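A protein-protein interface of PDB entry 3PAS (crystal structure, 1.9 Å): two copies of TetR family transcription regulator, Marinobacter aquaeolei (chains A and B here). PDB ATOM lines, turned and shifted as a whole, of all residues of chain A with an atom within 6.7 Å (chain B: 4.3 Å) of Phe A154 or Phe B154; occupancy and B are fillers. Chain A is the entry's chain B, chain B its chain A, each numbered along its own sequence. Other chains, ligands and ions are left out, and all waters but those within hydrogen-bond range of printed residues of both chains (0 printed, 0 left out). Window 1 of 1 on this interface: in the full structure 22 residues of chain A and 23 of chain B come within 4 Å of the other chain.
Phe A154 touches Pro B158, and with the chains exchanged Pro A158 touches Phe B154.
Phe A154 touches Met B184, and with the chains exchanged Met A184 touches Phe B154.
Phe A154 touches Ala B185, and with the chains exchanged Ala A185 touches Phe B154.
Met A184 touches Val B189, and with the chains exchanged Val A189 touches Met B184.
Positions printed for both chains: 150, 151, 152, 153, 154, 155, 156, 158, 181, 184, 185, 188 and 189.
The backbone carbonyl oxygen of Pro A149 lies within hydrogen-bond range of the side-chain hydroxyl of Thr A153 (2.7 Å).
Phe A154 touches just these residues of chain B: Phe B154 (3.5 Å), Pro B158 (3.7 Å), Ala B181 (3.4 Å), Met B184 (3.6 Å) and Ala B185 (3.8 Å).
Phe B154 touches just these residues of chain A: Phe A154 (3.5 Å), Pro A158 (3.7 Å), Ala A181 (3.7 Å), Met A184 (3.7 Å) and Ala A185 (3.8 Å).
Of the printed residues of chain B, Pro A158 touches Thr B153 and Phe B154.
Printed residues of chain B within 4 Å of His A161: Glu B152 and Thr B153.
The nearest printed residue of chain B that does not touch Phe A154 is Ala B188 (5.2 Å).
Of the 22 printed residues of chain A, 12 touch a printed residue of chain B.
Hydrophobic or aromatic side chains of chain A that line the printed part of chain B: Leu A150, Phe A154, Pro A158, His A161, Leu A162, Leu A180, Ala A181, Met A184, Ala A185, Ala A188 and Val A189.
Along chain A the printed residues that touch a printed residue of chain B span positions 150 to 189.
Printed residues of chain B that touch a printed residue of chain A: Leu B150, Glu B152, Thr B153, Phe B154, Pro B158, Ala B181, Met B184, Ala B185, Ala B188 and Val B189.
Among the printed residues, 25 pairs touch across the chains.
Among the printed residues, no Asp or Glu carboxylate lies within 4 Å of a Lys or Arg side-chain nitrogen of the other chain.
A ring nitrogen (NE2) of His A161 sits at hydrogen-bond distance from the side-chain carboxylate (OE1) of Glu B152.
Among the printed residues, merely in contact across the chains: Leu A150 with Ala B181 (3.8 Å), Leu A150 with Met B184 (3.6 Å), Thr A153 with Pro B158 (3.7 Å), Phe A154 with Phe B154 (3.5 Å), Phe A154 with Pro B158 (3.7 Å), Phe A154 with Ala B181 (3.4 Å), Phe A154 with Met B184 (3.6 Å), Phe A154 with Ala B185 (3.8 Å), Pro A158 with Thr B153 (3.7 Å), Pro A158 with Phe B154 (3.7 Å), His A161 with Thr B153 (3.2 Å), Leu A162 with Leu B150 (3.8 Å), Leu A162 with Thr B153 (3.4 Å), Leu A180 with Leu B150 (3.8 Å), Ala A181 with Leu B150 (3.9 Å), Ala A181 with Phe B154 (3.7 Å), Met A184 with Leu B150 (3.9 Å), Met A184 with Phe B154 (3.7 Å), Met A184 with Ala B188 (3.5 Å), Met A184 with Val B189 (3.9 Å), Ala A185 with Phe B154 (3.8 Å), Ala A188 with Met B184 (3.3 Å), Ala A188 with Ala B188 (3.8 Å) and Val A189 with Met B184 (3.9 Å).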
ATOM      1  N   TRP A  89      22.024 -24.712 -25.813  1.00  0.00           N
ATOM      2  CA  TRP A  89      20.867 -23.781 -25.826  1.00  0.00           C
ATOM      3  C   TRP A  89      21.233 -22.451 -25.262  1.00  0.00           C
ATOM      4  O   TRP A  89      20.959 -21.413 -25.878  1.00  0.00           O
ATOM      5  CB  TRP A  89      19.687 -24.374 -25.088  1.00  0.00           C
ATOM      6  CG  TRP A  89      18.539 -23.475 -24.807  1.00  0.00           C
ATOM      7  CD1 TRP A  89      18.469 -22.498 -23.869  1.00  0.00           C
ATOM      8  CD2 TRP A  89      17.270 -23.485 -25.473  1.00  0.00           C
ATOM      9  NE1 TRP A  89      17.252 -21.878 -23.928  1.00  0.00           N
ATOM     10  CE2 TRP A  89      16.491 -22.485 -24.890  1.00  0.00           C
ATOM     11  CE3 TRP A  89      16.720 -24.272 -26.495  1.00  0.00           C
ATOM     12  CZ2 TRP A  89      15.164 -22.231 -25.280  1.00  0.00           C
ATOM     13  CZ3 TRP A  89      15.442 -24.039 -26.877  1.00  0.00           C
ATOM     14  CH2 TRP A  89      14.652 -22.997 -26.258  1.00  0.00           C
ATOM     15  N   PRO A 149      12.023 -32.639 -38.481  1.00  0.00           N
ATOM     16  CA  PRO A 149      11.468 -31.283 -38.535  1.00  0.00           C
ATOM     17  C   PRO A 149      10.712 -30.865 -37.248  1.00  0.00           C
ATOM     18  O   PRO A 149      10.666 -29.662 -36.887  1.00  0.00           O
ATOM     19  CB  PRO A 149      10.529 -31.357 -39.726  1.00  0.00           C
ATOM     20  CG  PRO A 149      11.168 -32.412 -40.621  1.00  0.00           C
ATOM     21  CD  PRO A 149      11.704 -33.427 -39.686  1.00  0.00           C
ATOM     22  N   LEU A 150      10.120 -31.833 -36.553  1.00  0.00           N
ATOM     23  CA  LEU A 150       9.464 -31.548 -35.270  1.00  0.00           C
ATOM     24  C   LEU A 150      10.502 -31.217 -34.176  1.00  0.00           C
ATOM     25  O   LEU A 150      10.259 -30.362 -33.311  1.00  0.00           O
ATOM     26  CB  LEU A 150       8.540 -32.703 -34.840  1.00  0.00           C
ATOM     27  CG  LEU A 150       7.316 -33.014 -35.741  1.00  0.00           C
ATOM     28  CD1 LEU A 150       6.377 -34.034 -35.122  1.00  0.00           C
ATOM     29  CD2 LEU A 150       6.569 -31.724 -36.033  1.00  0.00           C
ATOM     30  N   LEU A 151      11.645 -31.907 -34.177  1.00  0.00           N
ATOM     31  CA  LEU A 151      12.711 -31.620 -33.249  1.00  0.00           C
ATOM     32  C   LEU A 151      13.247 -30.204 -33.474  1.00  0.00           C
ATOM     33  O   LEU A 151      13.451 -29.475 -32.510  1.00  0.00           O
ATOM     34  CB  LEU A 151      13.829 -32.651 -33.327  1.00  0.00           C
ATOM     35  CG  LEU A 151      13.442 -34.087 -32.909  1.00  0.00           C
ATOM     36  CD1 LEU A 151      14.747 -34.980 -32.966  1.00  0.00           C
ATOM     37  CD2 LEU A 151      12.738 -34.167 -31.516  1.00  0.00           C
ATOM     38  N   GLU A 152      13.429 -29.824 -34.736  1.00  0.00           N
ATOM     39  CA  GLU A 152      13.852 -28.467 -35.115  1.00  0.00           C
ATOM     40  C   GLU A 152      12.881 -27.428 -34.586  1.00  0.00           C
ATOM     41  O   GLU A 152      13.267 -26.403 -33.986  1.00  0.00           O
ATOM     42  CB  GLU A 152      13.961 -28.399 -36.648  1.00  0.00           C
ATOM     43  CG  GLU A 152      14.433 -27.095 -37.288  1.00  0.00           C
ATOM     44  CD  GLU A 152      13.330 -26.045 -37.455  1.00  0.00           C
ATOM     45  OE1 GLU A 152      12.201 -26.378 -37.907  1.00  0.00           O
ATOM     46  OE2 GLU A 152      13.613 -24.859 -37.200  1.00  0.00           O
ATOM     47  N   THR A 153      11.595 -27.714 -34.783  1.00  0.00           N
ATOM     48  CA  THR A 153      10.509 -26.812 -34.383  1.00  0.00           C
ATOM     49  C   THR A 153      10.452 -26.510 -32.899  1.00  0.00           C
ATOM     50  O   THR A 153      10.205 -25.338 -32.520  1.00  0.00           O
ATOM     51  CB  THR A 153       9.133 -27.379 -34.875  1.00  0.00           C
ATOM     52  OG1 THR A 153       9.192 -27.460 -36.312  1.00  0.00           O
ATOM     53  CG2 THR A 153       7.935 -26.497 -34.453  1.00  0.00           C
ATOM     54  N   PHE A 154      10.697 -27.528 -32.074  1.00  0.00           N
ATOM     55  CA  PHE A 154      10.553 -27.394 -30.640  1.00  0.00           C
ATOM     56  C   PHE A 154      11.861 -27.210 -29.853  1.00  0.00           C
ATOM     57  O   PHE A 154      11.796 -26.812 -28.708  1.00  0.00           O
ATOM     58  CB  PHE A 154       9.765 -28.571 -30.034  1.00  0.00           C
ATOM     59  CG  PHE A 154       8.301 -28.533 -30.395  1.00  0.00           C
ATOM     60  CD1 PHE A 154       7.448 -27.702 -29.718  1.00  0.00           C
ATOM     61  CD2 PHE A 154       7.809 -29.243 -31.493  1.00  0.00           C
ATOM     62  CE1 PHE A 154       6.100 -27.595 -30.061  1.00  0.00           C
ATOM     63  CE2 PHE A 154       6.449 -29.130 -31.880  1.00  0.00           C
ATOM     64  CZ  PHE A 154       5.580 -28.320 -31.153  1.00  0.00           C
ATOM     65  N   MET A 155      12.998 -27.540 -30.446  1.00  0.00           N
ATOM     66  CA  MET A 155      14.312 -27.444 -29.757  1.00  0.00           C
ATOM     67  C   MET A 155      15.262 -26.358 -30.318  1.00  0.00           C
ATOM     68  O   MET A 155      16.085 -25.836 -29.578  1.00  0.00           O
ATOM     69  CB  MET A 155      15.013 -28.796 -29.702  1.00  0.00           C
ATOM     70  CG  MET A 155      16.387 -28.880 -28.970  1.00  0.00           C
ATOM     71  SD  MET A 155      16.480 -28.174 -27.183  1.00  0.00           S
ATOM     72  CE  MET A 155      15.537 -29.665 -26.284  1.00  0.00           C
ATOM     73  N   PHE A 156      15.162 -26.000 -31.586  1.00  0.00           N
ATOM     74  CA  PHE A 156      16.067 -24.961 -32.137  1.00  0.00           C
ATOM     75  C   PHE A 156      15.371 -23.670 -32.512  1.00  0.00           C
ATOM     76  O   PHE A 156      15.785 -22.564 -32.121  1.00  0.00           O
ATOM     77  CB  PHE A 156      16.843 -25.576 -33.287  1.00  0.00           C
ATOM     78  CG  PHE A 156      17.651 -26.753 -32.853  1.00  0.00           C
ATOM     79  CD1 PHE A 156      18.881 -26.569 -32.240  1.00  0.00           C
ATOM     80  CD2 PHE A 156      17.149 -28.046 -32.970  1.00  0.00           C
ATOM     81  CE1 PHE A 156      19.608 -27.660 -31.801  1.00  0.00           C
ATOM     82  CE2 PHE A 156      17.886 -29.133 -32.542  1.00  0.00           C
ATOM     83  CZ  PHE A 156      19.117 -28.931 -31.956  1.00  0.00           C
ATOM     84  N   ARG A 157      14.246 -23.792 -33.200  1.00  0.00           N
ATOM     85  CA  ARG A 157      13.538 -22.613 -33.633  1.00  0.00           C
ATOM     86  C   ARG A 157      13.104 -21.720 -32.501  1.00  0.00           C
ATOM     87  O   ARG A 157      13.087 -20.520 -32.672  1.00  0.00           O
ATOM     88  CB  ARG A 157      12.300 -23.008 -34.449  1.00  0.00           C
ATOM     89  CG  ARG A 157      11.571 -21.872 -35.089  1.00  0.00           C
ATOM     90  CD  ARG A 157      12.471 -21.288 -36.147  1.00  0.00           C
ATOM     91  NE  ARG A 157      11.790 -20.305 -36.954  1.00  0.00           N
ATOM     92  CZ  ARG A 157      12.392 -19.594 -37.895  1.00  0.00           C
ATOM     93  NH1 ARG A 157      13.697 -19.749 -38.134  1.00  0.00           N
ATOM     94  NH2 ARG A 157      11.692 -18.715 -38.579  1.00  0.00           N
ATOM     95  N   PRO A 158      12.763 -22.283 -31.327  1.00  0.00           N
ATOM     96  CA  PRO A 158      12.312 -21.310 -30.312  1.00  0.00           C
ATOM     97  C   PRO A 158      13.393 -20.327 -29.830  1.00  0.00           C
ATOM     98  O   PRO A 158      13.036 -19.257 -29.316  1.00  0.00           O
ATOM     99  CB  PRO A 158      11.806 -22.194 -29.150  1.00  0.00           C
ATOM    100  CG  PRO A 158      11.419 -23.487 -29.840  1.00  0.00           C
ATOM    101  CD  PRO A 158      12.454 -23.662 -30.949  1.00  0.00           C
ATOM    102  N   HIS A 161      13.067 -17.306 -32.138  1.00  0.00           N
ATOM    103  CA  HIS A 161      11.832 -16.578 -31.803  1.00  0.00           C
ATOM    104  C   HIS A 161      11.962 -15.808 -30.497  1.00  0.00           C
ATOM    105  O   HIS A 161      11.606 -14.654 -30.440  1.00  0.00           O
ATOM    106  CB  HIS A 161      10.675 -17.576 -31.783  1.00  0.00           C
ATOM    107  CG  HIS A 161       9.333 -16.975 -31.514  1.00  0.00           C
ATOM    108  ND1 HIS A 161       8.651 -16.208 -32.443  1.00  0.00           N
ATOM    109  CD2 HIS A 161       8.535 -17.047 -30.417  1.00  0.00           C
ATOM    110  CE1 HIS A 161       7.491 -15.828 -31.920  1.00  0.00           C
ATOM    111  NE2 HIS A 161       7.390 -16.328 -30.693  1.00  0.00           N
ATOM    112  N   LEU A 162      12.528 -16.442 -29.467  1.00  0.00           N
ATOM    113  CA  LEU A 162      12.680 -15.808 -28.153  1.00  0.00           C
ATOM    114  C   LEU A 162      13.762 -14.731 -28.162  1.00  0.00           C
ATOM    115  O   LEU A 162      13.601 -13.682 -27.504  1.00  0.00           O
ATOM    116  CB  LEU A 162      12.947 -16.845 -27.083  1.00  0.00           C
ATOM    117  CG  LEU A 162      11.699 -17.690 -26.718  1.00  0.00           C
ATOM    118  CD1 LEU A 162      12.078 -18.925 -25.800  1.00  0.00           C
ATOM    119  CD2 LEU A 162      10.678 -16.835 -26.035  1.00  0.00           C
ATOM    120  N   LEU A 180      14.458 -21.650 -18.161  1.00  0.00           N
ATOM    121  CA  LEU A 180      13.061 -22.036 -18.142  1.00  0.00           C
ATOM    122  C   LEU A 180      12.565 -22.380 -19.552  1.00  0.00           C
ATOM    123  O   LEU A 180      11.900 -23.391 -19.755  1.00  0.00           O
ATOM    124  CB  LEU A 180      12.233 -20.905 -17.573  1.00  0.00           C
ATOM    125  CG  LEU A 180      10.714 -20.987 -17.630  1.00  0.00           C
ATOM    126  CD1 LEU A 180      10.230 -22.274 -16.903  1.00  0.00           C
ATOM    127  CD2 LEU A 180      10.172 -19.739 -16.940  1.00  0.00           C
ATOM    128  N   ALA A 181      12.923 -21.543 -20.524  1.00  0.00           N
ATOM    129  CA  ALA A 181      12.591 -21.819 -21.919  1.00  0.00           C
ATOM    130  C   ALA A 181      13.229 -23.146 -22.377  1.00  0.00           C
ATOM    131  O   ALA A 181      12.562 -23.952 -23.052  1.00  0.00           O
ATOM    132  CB  ALA A 181      13.110 -20.638 -22.809  1.00  0.00           C
ATOM    133  N   PHE A 182      14.500 -23.397 -22.025  1.00  0.00           N
ATOM    134  CA  PHE A 182      15.085 -24.702 -22.349  1.00  0.00           C
ATOM    135  C   PHE A 182      14.326 -25.859 -21.700  1.00  0.00           C
ATOM    136  O   PHE A 182      14.127 -26.903 -22.347  1.00  0.00           O
ATOM    137  CB  PHE A 182      16.595 -24.857 -21.991  1.00  0.00           C
ATOM    138  CG  PHE A 182      17.090 -26.288 -22.142  1.00  0.00           C
ATOM    139  CD1 PHE A 182      17.406 -26.760 -23.372  1.00  0.00           C
ATOM    140  CD2 PHE A 182      17.140 -27.173 -21.051  1.00  0.00           C
ATOM    141  CE1 PHE A 182      17.807 -28.092 -23.557  1.00  0.00           C
ATOM    142  CE2 PHE A 182      17.532 -28.503 -21.224  1.00  0.00           C
ATOM    143  CZ  PHE A 182      17.877 -28.951 -22.470  1.00  0.00           C
ATOM    144  N   ASN A 183      13.929 -25.705 -20.438  1.00  0.00           N
ATOM    145  CA  ASN A 183      13.149 -26.779 -19.787  1.00  0.00           C
ATOM    146  C   ASN A 183      11.835 -27.125 -20.539  1.00  0.00           C
ATOM    147  O   ASN A 183      11.445 -28.272 -20.628  1.00  0.00           O
ATOM    148  CB  ASN A 183      12.856 -26.442 -18.333  1.00  0.00           C
ATOM    149  CG  ASN A 183      14.126 -26.498 -17.460  1.00  0.00           C
ATOM    150  OD1 ASN A 183      15.112 -27.143 -17.822  1.00  0.00           O
ATOM    151  ND2 ASN A 183      14.119 -25.776 -16.366  1.00  0.00           N
ATOM    152  N   MET A 184      11.205 -26.103 -21.096  1.00  0.00           N
ATOM    153  CA  MET A 184      10.012 -26.281 -21.914  1.00  0.00           C
ATOM    154  C   MET A 184      10.346 -27.001 -23.217  1.00  0.00           C
ATOM    155  O   MET A 184       9.588 -27.916 -23.637  1.00  0.00           O
ATOM    156  CB  MET A 184       9.302 -24.948 -22.141  1.00  0.00           C
ATOM    157  CG  MET A 184       8.745 -24.399 -20.836  1.00  0.00           C
ATOM    158  SD  MET A 184       8.010 -22.672 -21.005  1.00  0.00           S
ATOM    159  CE  MET A 184       6.249 -23.194 -21.888  1.00  0.00           C
ATOM    160  N   ALA A 185      11.451 -26.602 -23.857  1.00  0.00           N
ATOM    161  CA  ALA A 185      11.897 -27.229 -25.112  1.00  0.00           C
ATOM    162  C   ALA A 185      12.234 -28.684 -24.885  1.00  0.00           C
ATOM    163  O   ALA A 185      11.825 -29.554 -25.671  1.00  0.00           O
ATOM    164  CB  ALA A 185      13.099 -26.500 -25.739  1.00  0.00           C
ATOM    165  N   TRP A 186      12.901 -28.989 -23.772  1.00  0.00           N
ATOM    166  CA  TRP A 186      13.216 -30.356 -23.423  1.00  0.00           C
ATOM    167  C   TRP A 186      11.958 -31.168 -23.194  1.00  0.00           C
ATOM    168  O   TRP A 186      11.780 -32.212 -23.768  1.00  0.00           O
ATOM    169  CB  TRP A 186      14.116 -30.428 -22.178  1.00  0.00           C
ATOM    170  CG  TRP A 186      14.336 -31.868 -21.748  1.00  0.00           C
ATOM    171  CD1 TRP A 186      13.729 -32.515 -20.721  1.00  0.00           C
ATOM    172  CD2 TRP A 186      15.228 -32.818 -22.347  1.00  0.00           C
ATOM    173  NE1 TRP A 186      14.173 -33.800 -20.653  1.00  0.00           N
ATOM    174  CE2 TRP A 186      15.070 -34.025 -21.649  1.00  0.00           C
ATOM    175  CE3 TRP A 186      16.079 -32.782 -23.462  1.00  0.00           C
ATOM    176  CZ2 TRP A 186      15.754 -35.192 -22.005  1.00  0.00           C
ATOM    177  CZ3 TRP A 186      16.745 -33.932 -23.825  1.00  0.00           C
ATOM    178  CH2 TRP A 186      16.592 -35.120 -23.085  1.00  0.00           C
ATOM    179  N   ALA A 188       9.095 -30.644 -24.429  1.00  0.00           N
ATOM    180  CA  ALA A 188       8.493 -30.842 -25.753  1.00  0.00           C
ATOM    181  C   ALA A 188       9.061 -32.086 -26.500  1.00  0.00           C
ATOM    182  O   ALA A 188       8.296 -32.881 -27.055  1.00  0.00           O
ATOM    183  CB  ALA A 188       8.711 -29.591 -26.635  1.00  0.00           C
ATOM    184  N   VAL A 189      10.390 -32.229 -26.501  1.00  0.00           N
ATOM    185  CA  VAL A 189      11.072 -33.283 -27.260  1.00  0.00           C
ATOM    186  C   VAL A 189      11.312 -34.609 -26.524  1.00  0.00           C
ATOM    187  O   VAL A 189      11.611 -35.628 -27.170  1.00  0.00           O
ATOM    188  CB  VAL A 189      12.411 -32.790 -27.879  1.00  0.00           C
ATOM    189  CG1 VAL A 189      12.158 -31.511 -28.736  1.00  0.00           C
ATOM    190  CG2 VAL A 189      13.499 -32.583 -26.813  1.00  0.00           C
ATOM    191  N   LEU B 150       6.222 -17.288 -23.475  1.00  0.00           N
ATOM    192  CA  LEU B 150       6.647 -18.651 -23.522  1.00  0.00           C
ATOM    193  C   LEU B 150       5.560 -19.608 -23.953  1.00  0.00           C
ATOM    194  O   LEU B 150       5.839 -20.553 -24.704  1.00  0.00           O
ATOM    195  CB  LEU B 150       7.230 -19.088 -22.184  1.00  0.00           C
ATOM    196  CG  LEU B 150       8.579 -18.442 -21.927  1.00  0.00           C
ATOM    197  CD1 LEU B 150       9.077 -18.784 -20.495  1.00  0.00           C
ATOM    198  CD2 LEU B 150       9.529 -18.992 -23.035  1.00  0.00           C
ATOM    199  N   LEU B 151       4.330 -19.397 -23.473  1.00  0.00           N
ATOM    200  CA  LEU B 151       3.226 -20.227 -23.874  1.00  0.00           C
ATOM    201  C   LEU B 151       2.991 -20.063 -25.362  1.00  0.00           C
ATOM    202  O   LEU B 151       2.818 -21.030 -26.045  1.00  0.00           O
ATOM    203  CB  LEU B 151       1.947 -19.908 -23.081  1.00  0.00           C
ATOM    204  CG  LEU B 151       1.975 -20.239 -21.596  1.00  0.00           C
ATOM    205  CD1 LEU B 151       0.649 -19.783 -20.880  1.00  0.00           C
ATOM    206  CD2 LEU B 151       2.298 -21.750 -21.366  1.00  0.00           C
ATOM    207  N   GLU B 152       3.009 -18.831 -25.851  1.00  0.00           N
ATOM    208  CA  GLU B 152       2.832 -18.513 -27.279  1.00  0.00           C
ATOM    209  C   GLU B 152       3.908 -19.187 -28.148  1.00  0.00           C
ATOM    210  O   GLU B 152       3.617 -19.758 -29.212  1.00  0.00           O
ATOM    211  CB  GLU B 152       2.917 -16.980 -27.472  1.00  0.00           C
ATOM    212  CG  GLU B 152       2.654 -16.495 -28.883  1.00  0.00           C
ATOM    213  CD  GLU B 152       3.917 -16.376 -29.794  1.00  0.00           C
ATOM    214  OE1 GLU B 152       5.056 -16.185 -29.322  1.00  0.00           O
ATOM    215  OE2 GLU B 152       3.730 -16.425 -31.005  1.00  0.00           O
ATOM    216  N   THR B 153       5.151 -19.112 -27.677  1.00  0.00           N
ATOM    217  CA  THR B 153       6.278 -19.766 -28.366  1.00  0.00           C
ATOM    218  C   THR B 153       6.091 -21.270 -28.567  1.00  0.00           C
ATOM    219  O   THR B 153       6.386 -21.809 -29.606  1.00  0.00           O
ATOM    220  CB  THR B 153       7.611 -19.466 -27.601  1.00  0.00           C
ATOM    221  OG1 THR B 153       7.827 -18.061 -27.519  1.00  0.00           O
ATOM    222  CG2 THR B 153       8.832 -20.085 -28.309  1.00  0.00           C
ATOM    223  N   PHE B 154       5.587 -21.970 -27.566  1.00  0.00           N
ATOM    224  CA  PHE B 154       5.524 -23.424 -27.641  1.00  0.00           C
ATOM    225  C   PHE B 154       4.145 -24.007 -28.008  1.00  0.00           C
ATOM    226  O   PHE B 154       4.110 -25.126 -28.540  1.00  0.00           O
ATOM    227  CB  PHE B 154       6.036 -24.053 -26.349  1.00  0.00           C
ATOM    228  CG  PHE B 154       7.502 -23.896 -26.152  1.00  0.00           C
ATOM    229  CD1 PHE B 154       8.397 -24.724 -26.834  1.00  0.00           C
ATOM    230  CD2 PHE B 154       8.013 -22.957 -25.290  1.00  0.00           C
ATOM    231  CE1 PHE B 154       9.749 -24.561 -26.682  1.00  0.00           C
ATOM    232  CE2 PHE B 154       9.374 -22.804 -25.137  1.00  0.00           C
ATOM    233  CZ  PHE B 154      10.230 -23.623 -25.855  1.00  0.00           C
ATOM    234  N   MET B 155       3.057 -23.246 -27.789  1.00  0.00           N
ATOM    235  CA  MET B 155       1.675 -23.738 -28.052  1.00  0.00           C
ATOM    236  C   MET B 155       1.029 -23.104 -29.276  1.00  0.00           C
ATOM    237  O   MET B 155       0.137 -23.686 -29.861  1.00  0.00           O
ATOM    238  CB  MET B 155       0.785 -23.494 -26.815  1.00  0.00           C
ATOM    239  CG  MET B 155      -0.709 -24.019 -26.893  1.00  0.00           C
ATOM    240  SD  MET B 155      -0.916 -25.835 -27.562  1.00  0.00           S
ATOM    241  CE  MET B 155      -0.456 -26.918 -26.062  1.00  0.00           C
ATOM    242  N   PHE B 156       1.452 -21.906 -29.679  1.00  0.00           N
ATOM    243  CA  PHE B 156       0.808 -21.278 -30.850  1.00  0.00           C
ATOM    244  C   PHE B 156       1.723 -21.101 -32.027  1.00  0.00           C
ATOM    245  O   PHE B 156       1.410 -21.487 -33.138  1.00  0.00           O
ATOM    246  CB  PHE B 156       0.171 -19.941 -30.474  1.00  0.00           C
ATOM    247  CG  PHE B 156      -0.885 -20.056 -29.389  1.00  0.00           C
ATOM    248  CD1 PHE B 156      -2.173 -20.475 -29.697  1.00  0.00           C
ATOM    249  CD2 PHE B 156      -0.587 -19.759 -28.071  1.00  0.00           C
ATOM    250  CE1 PHE B 156      -3.133 -20.601 -28.692  1.00  0.00           C
ATOM    251  CE2 PHE B 156      -1.540 -19.873 -27.062  1.00  0.00           C
ATOM    252  CZ  PHE B 156      -2.806 -20.295 -27.369  1.00  0.00           C
ATOM    253  N   PRO B 158       4.449 -22.665 -33.093  1.00  0.00           N
ATOM    254  CA  PRO B 158       4.824 -23.784 -33.980  1.00  0.00           C
ATOM    255  C   PRO B 158       3.831 -24.153 -35.110  1.00  0.00           C
ATOM    256  O   PRO B 158       4.255 -24.697 -36.114  1.00  0.00           O
ATOM    257  CB  PRO B 158       4.939 -24.961 -33.039  1.00  0.00           C
ATOM    258  CG  PRO B 158       5.220 -24.318 -31.648  1.00  0.00           C
ATOM    259  CD  PRO B 158       4.308 -23.100 -31.691  1.00  0.00           C
ATOM    260  N   ALA B 181       2.990 -33.223 -33.269  1.00  0.00           N
ATOM    261  CA  ALA B 181       3.397 -31.844 -32.953  1.00  0.00           C
ATOM    262  C   ALA B 181       2.599 -31.283 -31.769  1.00  0.00           C
ATOM    263  O   ALA B 181       3.152 -30.681 -30.831  1.00  0.00           O
ATOM    264  CB  ALA B 181       3.274 -30.920 -34.243  1.00  0.00           C
ATOM    265  N   MET B 184       3.768 -32.651 -28.460  1.00  0.00           N
ATOM    266  CA  MET B 184       4.960 -31.958 -28.055  1.00  0.00           C
ATOM    267  C   MET B 184       4.676 -30.556 -27.474  1.00  0.00           C
ATOM    268  O   MET B 184       5.250 -30.175 -26.447  1.00  0.00           O
ATOM    269  CB  MET B 184       5.943 -31.910 -29.251  1.00  0.00           C
ATOM    270  CG  MET B 184       6.371 -33.281 -29.676  1.00  0.00           C
ATOM    271  SD  MET B 184       7.261 -33.262 -31.399  1.00  0.00           S
ATOM    272  CE  MET B 184       8.983 -32.604 -30.734  1.00  0.00           C
ATOM    273  N   ALA B 185       3.776 -29.800 -28.099  1.00  0.00           N
ATOM    274  CA  ALA B 185       3.348 -28.502 -27.577  1.00  0.00           C
ATOM    275  C   ALA B 185       2.725 -28.662 -26.215  1.00  0.00           C
ATOM    276  O   ALA B 185       3.030 -27.901 -25.295  1.00  0.00           O
ATOM    277  CB  ALA B 185       2.329 -27.771 -28.578  1.00  0.00           C
ATOM    278  N   ALA B 188       5.391 -29.417 -23.583  1.00  0.00           N
ATOM    279  CA  ALA B 188       6.134 -28.201 -23.330  1.00  0.00           C
ATOM    280  C   ALA B 188       5.464 -27.306 -22.295  1.00  0.00           C
ATOM    281  O   ALA B 188       6.134 -26.769 -21.398  1.00  0.00           O
ATOM    282  CB  ALA B 188       6.280 -27.416 -24.628  1.00  0.00           C
ATOM    283  N   VAL B 189       4.143 -27.163 -22.407  1.00  0.00           N
ATOM    284  CA  VAL B 189       3.427 -26.222 -21.533  1.00  0.00           C
ATOM    285  C   VAL B 189       2.831 -26.828 -20.291  1.00  0.00           C
ATOM    286  O   VAL B 189       2.484 -26.083 -19.371  1.00  0.00           O
ATOM    287  CB  VAL B 189       2.370 -25.409 -22.265  1.00  0.00           C
ATOM    288  CG1 VAL B 189       2.995 -24.650 -23.407  1.00  0.00           C
ATOM    289  CG2 VAL B 189       1.164 -26.263 -22.686  1.00  0.00           C
